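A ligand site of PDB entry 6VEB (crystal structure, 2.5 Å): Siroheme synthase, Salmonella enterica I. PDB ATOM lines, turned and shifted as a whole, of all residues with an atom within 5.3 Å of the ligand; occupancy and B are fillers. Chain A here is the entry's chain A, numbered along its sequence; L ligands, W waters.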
ATOM      1  N   PRO A 225     -22.541  19.546 -26.046  1.00  0.00           N
ATOM      2  CA  PRO A 225     -22.428  18.089 -26.077  1.00  0.00           C
ATOM      3  C   PRO A 225     -23.729  17.312 -25.869  1.00  0.00           C
ATOM      4  O   PRO A 225     -23.671  16.077 -25.842  1.00  0.00           O
ATOM      5  CB  PRO A 225     -21.456  17.803 -24.915  1.00  0.00           C
ATOM      6  CG  PRO A 225     -21.274  19.106 -24.164  1.00  0.00           C
ATOM      7  CD  PRO A 225     -22.245  20.080 -24.707  1.00  0.00           C
ATOM      8  N   GLY A 226     -24.881  17.963 -25.719  1.00  0.00           N
ATOM      9  CA  GLY A 226     -26.144  17.230 -25.618  1.00  0.00           C
ATOM     10  C   GLY A 226     -27.246  17.823 -24.738  1.00  0.00           C
ATOM     11  O   GLY A 226     -28.368  18.040 -25.211  1.00  0.00           O
ATOM     12  N   LEU A 250     -24.365  13.905 -33.471  1.00  0.00           N
ATOM     13  CA  LEU A 250     -24.033  14.248 -32.080  1.00  0.00           C
ATOM     14  C   LEU A 250     -24.773  15.467 -31.573  1.00  0.00           C
ATOM     15  O   LEU A 250     -24.487  15.944 -30.468  1.00  0.00           O
ATOM     16  CB  LEU A 250     -22.533  14.465 -31.870  1.00  0.00           C
ATOM     17  CG  LEU A 250     -21.598  13.277 -32.029  1.00  0.00           C
ATOM     18  CD1 LEU A 250     -20.511  13.703 -32.976  1.00  0.00           C
ATOM     19  CD2 LEU A 250     -21.057  12.830 -30.716  1.00  0.00           C
ATOM     20  N   GLY A 301     -22.348  19.202 -33.168  1.00  0.00           N
ATOM     21  CA  GLY A 301     -22.108  18.774 -31.806  1.00  0.00           C
ATOM     22  C   GLY A 301     -20.936  19.496 -31.169  1.00  0.00           C
ATOM     23  O   GLY A 301     -19.897  19.721 -31.795  1.00  0.00           O
ATOM     24  N   GLY A 302     -21.101  19.845 -29.892  1.00  0.00           N
ATOM     25  CA  GLY A 302     -20.025  20.497 -29.146  1.00  0.00           C
ATOM     26  C   GLY A 302     -19.654  21.836 -29.754  1.00  0.00           C
ATOM     27  O   GLY A 302     -20.501  22.714 -30.004  1.00  0.00           O
ATOM     28  N   ASP A 303     -18.369  22.012 -29.989  1.00  0.00           N
ATOM     29  CA  ASP A 303     -17.989  23.258 -30.594  1.00  0.00           C
ATOM     30  C   ASP A 303     -17.651  23.029 -32.070  1.00  0.00           C
ATOM     31  O   ASP A 303     -17.139  21.972 -32.423  1.00  0.00           O
ATOM     32  CB  ASP A 303     -16.794  23.856 -29.855  1.00  0.00           C
ATOM     33  CG  ASP A 303     -16.332  25.174 -30.477  1.00  0.00           C
ATOM     34  OD1 ASP A 303     -16.790  26.242 -30.044  1.00  0.00           O
ATOM     35  OD2 ASP A 303     -15.518  25.136 -31.422  1.00  0.00           O
ATOM     36  N   PRO A 304     -17.938  23.986 -32.964  1.00  0.00           N
ATOM     37  CA  PRO A 304     -17.673  23.748 -34.403  1.00  0.00           C
ATOM     38  C   PRO A 304     -16.189  23.714 -34.792  1.00  0.00           C
ATOM     39  O   PRO A 304     -15.846  23.051 -35.774  1.00  0.00           O
ATOM     40  CB  PRO A 304     -18.409  24.913 -35.104  1.00  0.00           C
ATOM     41  CG  PRO A 304     -19.372  25.453 -34.067  1.00  0.00           C
ATOM     42  CD  PRO A 304     -18.724  25.228 -32.731  1.00  0.00           C
ATOM     43  N   ILE A 306     -13.506  22.712 -32.858  1.00  0.00           N
ATOM     44  CA  ILE A 306     -12.718  21.688 -32.178  1.00  0.00           C
ATOM     45  C   ILE A 306     -13.123  20.346 -32.773  1.00  0.00           C
ATOM     46  O   ILE A 306     -14.107  19.740 -32.319  1.00  0.00           O
ATOM     47  CB  ILE A 306     -12.938  21.735 -30.660  1.00  0.00           C
ATOM     48  CG1 ILE A 306     -12.552  23.118 -30.111  1.00  0.00           C
ATOM     49  CG2 ILE A 306     -12.190  20.577 -29.985  1.00  0.00           C
ATOM     50  CD1 ILE A 306     -12.358  23.182 -28.601  1.00  0.00           C
ATOM     51  N   PHE A 307     -12.374  19.874 -33.773  1.00  0.00           N
ATOM     52  CA  PHE A 307     -12.618  18.579 -34.445  1.00  0.00           C
ATOM     53  C   PHE A 307     -14.052  18.506 -34.983  1.00  0.00           C
ATOM     54  O   PHE A 307     -14.710  17.467 -34.896  1.00  0.00           O
ATOM     55  CB  PHE A 307     -12.336  17.373 -33.532  1.00  0.00           C
ATOM     56  CG  PHE A 307     -10.962  17.374 -32.947  1.00  0.00           C
ATOM     57  CD1 PHE A 307      -9.826  17.336 -33.777  1.00  0.00           C
ATOM     58  CD2 PHE A 307     -10.789  17.452 -31.564  1.00  0.00           C
ATOM     59  CE1 PHE A 307      -8.538  17.352 -33.225  1.00  0.00           C
ATOM     60  CE2 PHE A 307      -9.498  17.486 -30.997  1.00  0.00           C
ATOM     61  CZ  PHE A 307      -8.376  17.448 -31.830  1.00  0.00           C
ATOM     62  N   GLY A 308     -14.543  19.621 -35.516  1.00  0.00           N
ATOM     63  CA  GLY A 308     -15.869  19.644 -36.093  1.00  0.00           C
ATOM     64  C   GLY A 308     -15.794  19.772 -37.593  1.00  0.00           C
ATOM     65  O   GLY A 308     -16.817  19.686 -38.280  1.00  0.00           O
ATOM     66  N   ILE A 330     -20.215  24.680 -26.248  1.00  0.00           N
ATOM     67  CA  ILE A 330     -19.535  23.932 -25.190  1.00  0.00           C
ATOM     68  C   ILE A 330     -18.954  22.647 -25.790  1.00  0.00           C
ATOM     69  O   ILE A 330     -19.686  21.723 -26.144  1.00  0.00           O
ATOM     70  CB  ILE A 330     -20.498  23.608 -24.035  1.00  0.00           C
ATOM     71  CG1 ILE A 330     -21.142  24.886 -23.445  1.00  0.00           C
ATOM     72  CG2 ILE A 330     -19.789  22.671 -22.989  1.00  0.00           C
ATOM     73  CD1 ILE A 330     -20.211  25.902 -22.833  1.00  0.00           C
ATOM     74  N   THR A 331     -17.623  22.584 -25.888  1.00  0.00           N
ATOM     75  CA  THR A 331     -16.966  21.374 -26.384  1.00  0.00           C
ATOM     76  C   THR A 331     -17.083  20.251 -25.355  1.00  0.00           C
ATOM     77  O   THR A 331     -17.334  20.479 -24.164  1.00  0.00           O
ATOM     78  CB  THR A 331     -15.498  21.656 -26.733  1.00  0.00           C
ATOM     79  OG1 THR A 331     -14.987  20.595 -27.552  1.00  0.00           O
ATOM     80  CG2 THR A 331     -14.646  21.792 -25.468  1.00  0.00           C
ATOM     81  N   ALA A 332     -16.879  19.022 -25.838  1.00  0.00           N
ATOM     82  CA  ALA A 332     -17.110  17.838 -25.004  1.00  0.00           C
ATOM     83  C   ALA A 332     -16.250  17.841 -23.758  1.00  0.00           C
ATOM     84  O   ALA A 332     -16.719  17.464 -22.667  1.00  0.00           O
ATOM     85  CB  ALA A 332     -16.844  16.561 -25.811  1.00  0.00           C
ATOM     86  N   ALA A 333     -14.984  18.280 -23.880  1.00  0.00           N
ATOM     87  CA  ALA A 333     -14.079  18.304 -22.737  1.00  0.00           C
ATOM     88  C   ALA A 333     -14.643  19.183 -21.609  1.00  0.00           C
ATOM     89  O   ALA A 333     -14.630  18.794 -20.429  1.00  0.00           O
ATOM     90  CB  ALA A 333     -12.701  18.778 -23.188  1.00  0.00           C
ATOM     91  N   CYS A 336     -17.959  17.460 -20.342  1.00  0.00           N
ATOM     92  CA  CYS A 336     -17.676  16.251 -19.562  1.00  0.00           C
ATOM     93  C   CYS A 336     -16.817  16.556 -18.348  1.00  0.00           C
ATOM     94  O   CYS A 336     -16.967  15.889 -17.315  1.00  0.00           O
ATOM     95  CB  CYS A 336     -17.033  15.178 -20.451  1.00  0.00           C
ATOM     96  SG  CYS A 336     -18.113  14.613 -21.912  1.00  0.00           S
ATOM     97  N   PHE A 380      -9.034  12.749 -25.024  1.00  0.00           N
ATOM     98  CA  PHE A 380      -9.080  12.141 -26.337  1.00  0.00           C
ATOM     99  C   PHE A 380     -10.513  12.200 -26.866  1.00  0.00           C
ATOM    100  O   PHE A 380     -11.441  11.649 -26.251  1.00  0.00           O
ATOM    101  CB  PHE A 380      -8.585  10.704 -26.299  1.00  0.00           C
ATOM    102  CG  PHE A 380      -7.149  10.579 -25.935  1.00  0.00           C
ATOM    103  CD1 PHE A 380      -6.186  10.425 -26.914  1.00  0.00           C
ATOM    104  CD2 PHE A 380      -6.758  10.608 -24.612  1.00  0.00           C
ATOM    105  CE1 PHE A 380      -4.852  10.316 -26.585  1.00  0.00           C
ATOM    106  CE2 PHE A 380      -5.427  10.510 -24.268  1.00  0.00           C
ATOM    107  CZ  PHE A 380      -4.471  10.361 -25.251  1.00  0.00           C
ATOM    108  N   TYR A 381     -10.690  12.883 -27.990  1.00  0.00           N
ATOM    109  CA  TYR A 381     -11.907  12.805 -28.780  1.00  0.00           C
ATOM    110  C   TYR A 381     -11.770  11.680 -29.796  1.00  0.00           C
ATOM    111  O   TYR A 381     -10.686  11.478 -30.353  1.00  0.00           O
ATOM    112  CB  TYR A 381     -12.157  14.118 -29.524  1.00  0.00           C
ATOM    113  CG  TYR A 381     -12.473  15.323 -28.681  1.00  0.00           C
ATOM    114  CD1 TYR A 381     -11.555  15.833 -27.740  1.00  0.00           C
ATOM    115  CD2 TYR A 381     -13.685  15.987 -28.875  1.00  0.00           C
ATOM    116  CE1 TYR A 381     -11.868  16.949 -26.996  1.00  0.00           C
ATOM    117  CE2 TYR A 381     -14.006  17.113 -28.128  1.00  0.00           C
ATOM    118  CZ  TYR A 381     -13.112  17.583 -27.203  1.00  0.00           C
ATOM    119  OH  TYR A 381     -13.471  18.698 -26.482  1.00  0.00           O
ATOM    120  N   MET A 382     -12.883  10.985 -30.066  1.00  0.00           N
ATOM    121  CA  MET A 382     -12.918   9.919 -31.065  1.00  0.00           C
ATOM    122  C   MET A 382     -11.855   8.861 -30.788  1.00  0.00           C
ATOM    123  O   MET A 382     -11.131   8.443 -31.683  1.00  0.00           O
ATOM    124  CB  MET A 382     -12.733  10.481 -32.488  1.00  0.00           C
ATOM    125  CG  MET A 382     -13.774  11.464 -32.980  1.00  0.00           C
ATOM    126  SD  MET A 382     -13.274  12.288 -34.539  1.00  0.00           S
ATOM    127  CE  MET A 382     -11.998  13.442 -33.985  1.00  0.00           C
ATOM    128  N   GLY A 383     -11.733   8.450 -29.516  1.00  0.00           N
ATOM    129  CA  GLY A 383     -10.620   7.588 -29.125  1.00  0.00           C
ATOM    130  C   GLY A 383     -11.013   6.232 -28.547  1.00  0.00           C
ATOM    131  O   GLY A 383     -10.152   5.422 -28.204  1.00  0.00           O
ATOM    132  N   VAL A 408     -16.106   9.216 -20.107  1.00  0.00           N
ATOM    133  CA  VAL A 408     -17.447   9.780 -19.982  1.00  0.00           C
ATOM    134  C   VAL A 408     -18.208   9.463 -21.248  1.00  0.00           C
ATOM    135  O   VAL A 408     -17.827   9.901 -22.341  1.00  0.00           O
ATOM    136  CB  VAL A 408     -17.422  11.288 -19.704  1.00  0.00           C
ATOM    137  CG1 VAL A 408     -18.809  11.752 -19.338  1.00  0.00           C
ATOM    138  CG2 VAL A 408     -16.409  11.611 -18.589  1.00  0.00           C
ATOM    139  N   GLU A 409     -19.280   8.683 -21.118  1.00  0.00           N
ATOM    140  CA  GLU A 409     -20.121   8.319 -22.250  1.00  0.00           C
ATOM    141  C   GLU A 409     -21.410   9.130 -22.218  1.00  0.00           C
ATOM    142  O   GLU A 409     -22.101   9.170 -21.207  1.00  0.00           O
ATOM    143  CB  GLU A 409     -20.426   6.824 -22.198  1.00  0.00           C
ATOM    144  CG  GLU A 409     -21.597   6.378 -23.022  1.00  0.00           C
ATOM    145  CD  GLU A 409     -22.076   4.990 -22.604  1.00  0.00           C
ATOM    146  OE1 GLU A 409     -22.755   4.874 -21.569  1.00  0.00           O
ATOM    147  OE2 GLU A 409     -21.731   4.013 -23.311  1.00  0.00           O
ATOM    148  N   ASN A 410     -21.716   9.792 -23.348  1.00  0.00           N
ATOM    149  CA  ASN A 410     -22.879  10.675 -23.457  1.00  0.00           C
ATOM    150  C   ASN A 410     -22.860  11.750 -22.357  1.00  0.00           C
ATOM    151  O   ASN A 410     -23.813  11.904 -21.573  1.00  0.00           O
ATOM    152  CB  ASN A 410     -24.185   9.862 -23.411  1.00  0.00           C
ATOM    153  CG  ASN A 410     -24.391   9.010 -24.635  1.00  0.00           C
ATOM    154  OD1 ASN A 410     -24.228   9.460 -25.764  1.00  0.00           O
ATOM    155  ND2 ASN A 410     -24.790   7.774 -24.423  1.00  0.00           N
ATOM    156  N   GLY A 411     -21.749  12.497 -22.307  1.00  0.00           N
ATOM    157  CA  GLY A 411     -21.577  13.491 -21.262  1.00  0.00           C
ATOM    158  C   GLY A 411     -22.642  14.590 -21.346  1.00  0.00           C
ATOM    159  O   GLY A 411     -22.996  15.047 -22.435  1.00  0.00           O
ATOM    160  N   THR A 412     -23.159  14.995 -20.181  1.00  0.00           N
ATOM    161  CA  THR A 412     -24.169  16.028 -19.935  1.00  0.00           C
ATOM    162  C   THR A 412     -25.579  15.522 -20.222  1.00  0.00           C
ATOM    163  O   THR A 412     -26.541  16.232 -19.929  1.00  0.00           O
ATOM    164  CB  THR A 412     -23.943  17.333 -20.729  1.00  0.00           C
ATOM    165  OG1 THR A 412     -24.278  17.111 -22.117  1.00  0.00           O
ATOM    166  CG2 THR A 412     -22.486  17.851 -20.611  1.00  0.00           C
ATOM    167  N   PRO A 436     -20.905   8.266 -28.157  1.00  0.00           N
ATOM    168  CA  PRO A 436     -19.768   9.179 -28.017  1.00  0.00           C
ATOM    169  C   PRO A 436     -19.174   9.143 -26.624  1.00  0.00           C
ATOM    170  O   PRO A 436     -19.900   9.286 -25.629  1.00  0.00           O
ATOM    171  CB  PRO A 436     -20.393  10.538 -28.304  1.00  0.00           C
ATOM    172  CG  PRO A 436     -21.775  10.409 -27.742  1.00  0.00           C
ATOM    173  CD  PRO A 436     -22.194   8.965 -27.987  1.00  0.00           C
ATOM    174  N   ALA A 437     -17.862   8.958 -26.534  1.00  0.00           N
ATOM    175  CA  ALA A 437     -17.210   8.978 -25.239  1.00  0.00           C
ATOM    176  C   ALA A 437     -15.881   9.706 -25.345  1.00  0.00           C
ATOM    177  O   ALA A 437     -15.206   9.678 -26.381  1.00  0.00           O
ATOM    178  CB  ALA A 437     -17.023   7.559 -24.685  1.00  0.00           C
ATOM    179  N   LEU A 438     -15.524  10.370 -24.252  1.00  0.00           N
ATOM    180  CA  LEU A 438     -14.298  11.123 -24.104  1.00  0.00           C
ATOM    181  C   LEU A 438     -13.379  10.402 -23.141  1.00  0.00           C
ATOM    182  O   LEU A 438     -13.844   9.899 -22.112  1.00  0.00           O
ATOM    183  CB  LEU A 438     -14.612  12.510 -23.569  1.00  0.00           C
ATOM    184  CG  LEU A 438     -13.853  13.717 -24.055  1.00  0.00           C
ATOM    185  CD1 LEU A 438     -13.975  13.927 -25.560  1.00  0.00           C
ATOM    186  CD2 LEU A 438     -14.467  14.870 -23.299  1.00  0.00           C
HETATM  187  N1  LIG L   1     -16.803  19.212 -32.131  1.00  0.00           N
HETATM  188  C1  LIG L   1     -17.122  18.319 -31.035  1.00  0.00           C
HETATM  189  C2  LIG L   1     -16.408  16.999 -31.233  1.00  0.00           C
HETATM  190  C3  LIG L   1     -16.600  16.371 -32.605  1.00  0.00           C
HETATM  191  S1  LIG L   1     -15.491  14.959 -32.866  1.00  0.00           S
HETATM  192  C4  LIG L   1     -16.756  18.977 -29.701  1.00  0.00           C
HETATM  193  O1  LIG L   1     -16.304  20.128 -29.693  1.00  0.00           O
HETATM  194  O2  LIG L   1     -16.920  18.395 -28.618  1.00  0.00           O
HETATM  195  C5  LIG L   1     -16.634  13.757 -32.108  1.00  0.00           C
HETATM  196  C6  LIG L   1     -16.140  13.250 -30.766  1.00  0.00           C
HETATM  197  O3  LIG L   1     -16.557  14.100 -29.706  1.00  0.00           O
HETATM  198  C7  LIG L   1     -16.687  11.879 -30.401  1.00  0.00           C
HETATM  199  O4  LIG L   1     -15.854  10.851 -30.829  1.00  0.00           O
HETATM  200  C8  LIG L   1     -16.663  11.857 -28.899  1.00  0.00           C
HETATM  201  O5  LIG L   1     -15.391  11.398 -28.484  1.00  0.00           O
HETATM  202  C9  LIG L   1     -16.759  13.318 -28.534  1.00  0.00           C
HETATM  203  N2  LIG L   1     -18.056  13.646 -27.916  1.00  0.00           N
HETATM  204  C10 LIG L   1     -19.037  14.435 -28.460  1.00  0.00           C
HETATM  205  N3  LIG L   1     -20.093  14.515 -27.602  1.00  0.00           N
HETATM  206  C11 LIG L   1     -19.792  13.796 -26.508  1.00  0.00           C
HETATM  207  C12 LIG L   1     -20.494  13.549 -25.328  1.00  0.00           C
HETATM  208  N4  LIG L   1     -21.704  14.097 -25.111  1.00  0.00           N
HETATM  209  N5  LIG L   1     -19.908  12.754 -24.361  1.00  0.00           N
HETATM  210  C13 LIG L   1     -18.666  12.224 -24.595  1.00  0.00           C
HETATM  211  N6  LIG L   1     -17.980  12.477 -25.770  1.00  0.00           N
HETATM  212  C14 LIG L   1     -18.529  13.237 -26.706  1.00  0.00           C
HETATM  213  O   HOH W   1     -16.637   8.418 -29.271  1.00  0.00           O
HETATM  214  O   HOH W   2     -22.049  15.858 -29.168  1.00  0.00           O
HETATM  215  O   HOH W   3     -18.671  18.779 -33.962  1.00  0.00           O
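O of Gly 301 sits at hydrogen-bond distance from N1 of the ligand (3.2 Å). The backbone carbonyl oxygen (O) of Pro 225 sits at hydrogen-bond distance from a nitrogen (N4) of the ligand (2.9 Å). N of Met 382 sits at hydrogen-bond distance from O5 of the ligand, 3.0 Å away. N of Ala 332 lies within hydrogen-bond range of O2 of the ligand (2.9 Å). N5 of the ligand lies within hydrogen-bond range of SG of Cys 336. The backbone carbonyl oxygen of Ala 437 is in hydrogen-bond range of an oxygen (O5) of the ligand (2.7 Å). N1 of the ligand lies within hydrogen-bond range of O of Ile 306 (2.8 Å). N of Asp 303 sits at hydrogen-bond distance from O1 of the ligand (2.8 Å). N of Gly 411 lies within hydrogen-bond range of N5 of the ligand, 2.8 Å away. A nitrogen (N1) of the ligand sits at hydrogen-bond distance from the backbone carbonyl oxygen (O) of Asp 303, 2.8 Å away. OG1 of Thr 331 is in hydrogen-bond range of O1 of the ligand. O of Gly 411 lies within hydrogen-bond range of N4 of the ligand, at 3.1 Å.
The backbone NH (N) of Ala 332 is in hydrogen-bond range of the side-chain hydroxyl (OH) of Tyr 381, at 3.5 Å. SG of Cys 336 sits close to O of Ala 332 (3.3 Å). The side-chain hydroxyl (OG1) of Thr 331 lies within hydrogen-bond range of the side-chain hydroxyl (OH) of Tyr 381 (2.7 Å). The backbone NH (N) of Ile 306 sits at hydrogen-bond distance from the side-chain carboxylate (OD2) of Asp 303 (3.5 Å). O of Val 408 lies within hydrogen-bond range of N of Leu 438. The backbone carbonyl oxygen of Pro 436 lies within hydrogen-bond range of the backbone NH of Asn 410. N of Ala 333 lies within hydrogen-bond range of OH of Tyr 381, 3.0 Å away.
The backbone carbonyl oxygen (O) of Phe 307 lies close to a sulfur (S1) of the ligand (3.3 Å). Merely in contact with the ligand: Tyr 381, Val 408, Pro 436, Leu 250, Leu 438, Asn 410 and Gly 302. Of the 27 residues printed, 18 come within 4 Å of the ligand.
Water W3 lies within hydrogen-bond range of N1 of the ligand (2.7 Å) and O of Gly 301 (2.7 Å). Water W2 bridges the backbone carbonyl oxygen (O) of Leu 250 (2.8 Å) and a nitrogen (N3) of the ligand (2.8 Å). Water W1 lies within hydrogen-bond range of O4 of the ligand (3.0 Å) and N of Ala 437 (3.0 Å).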
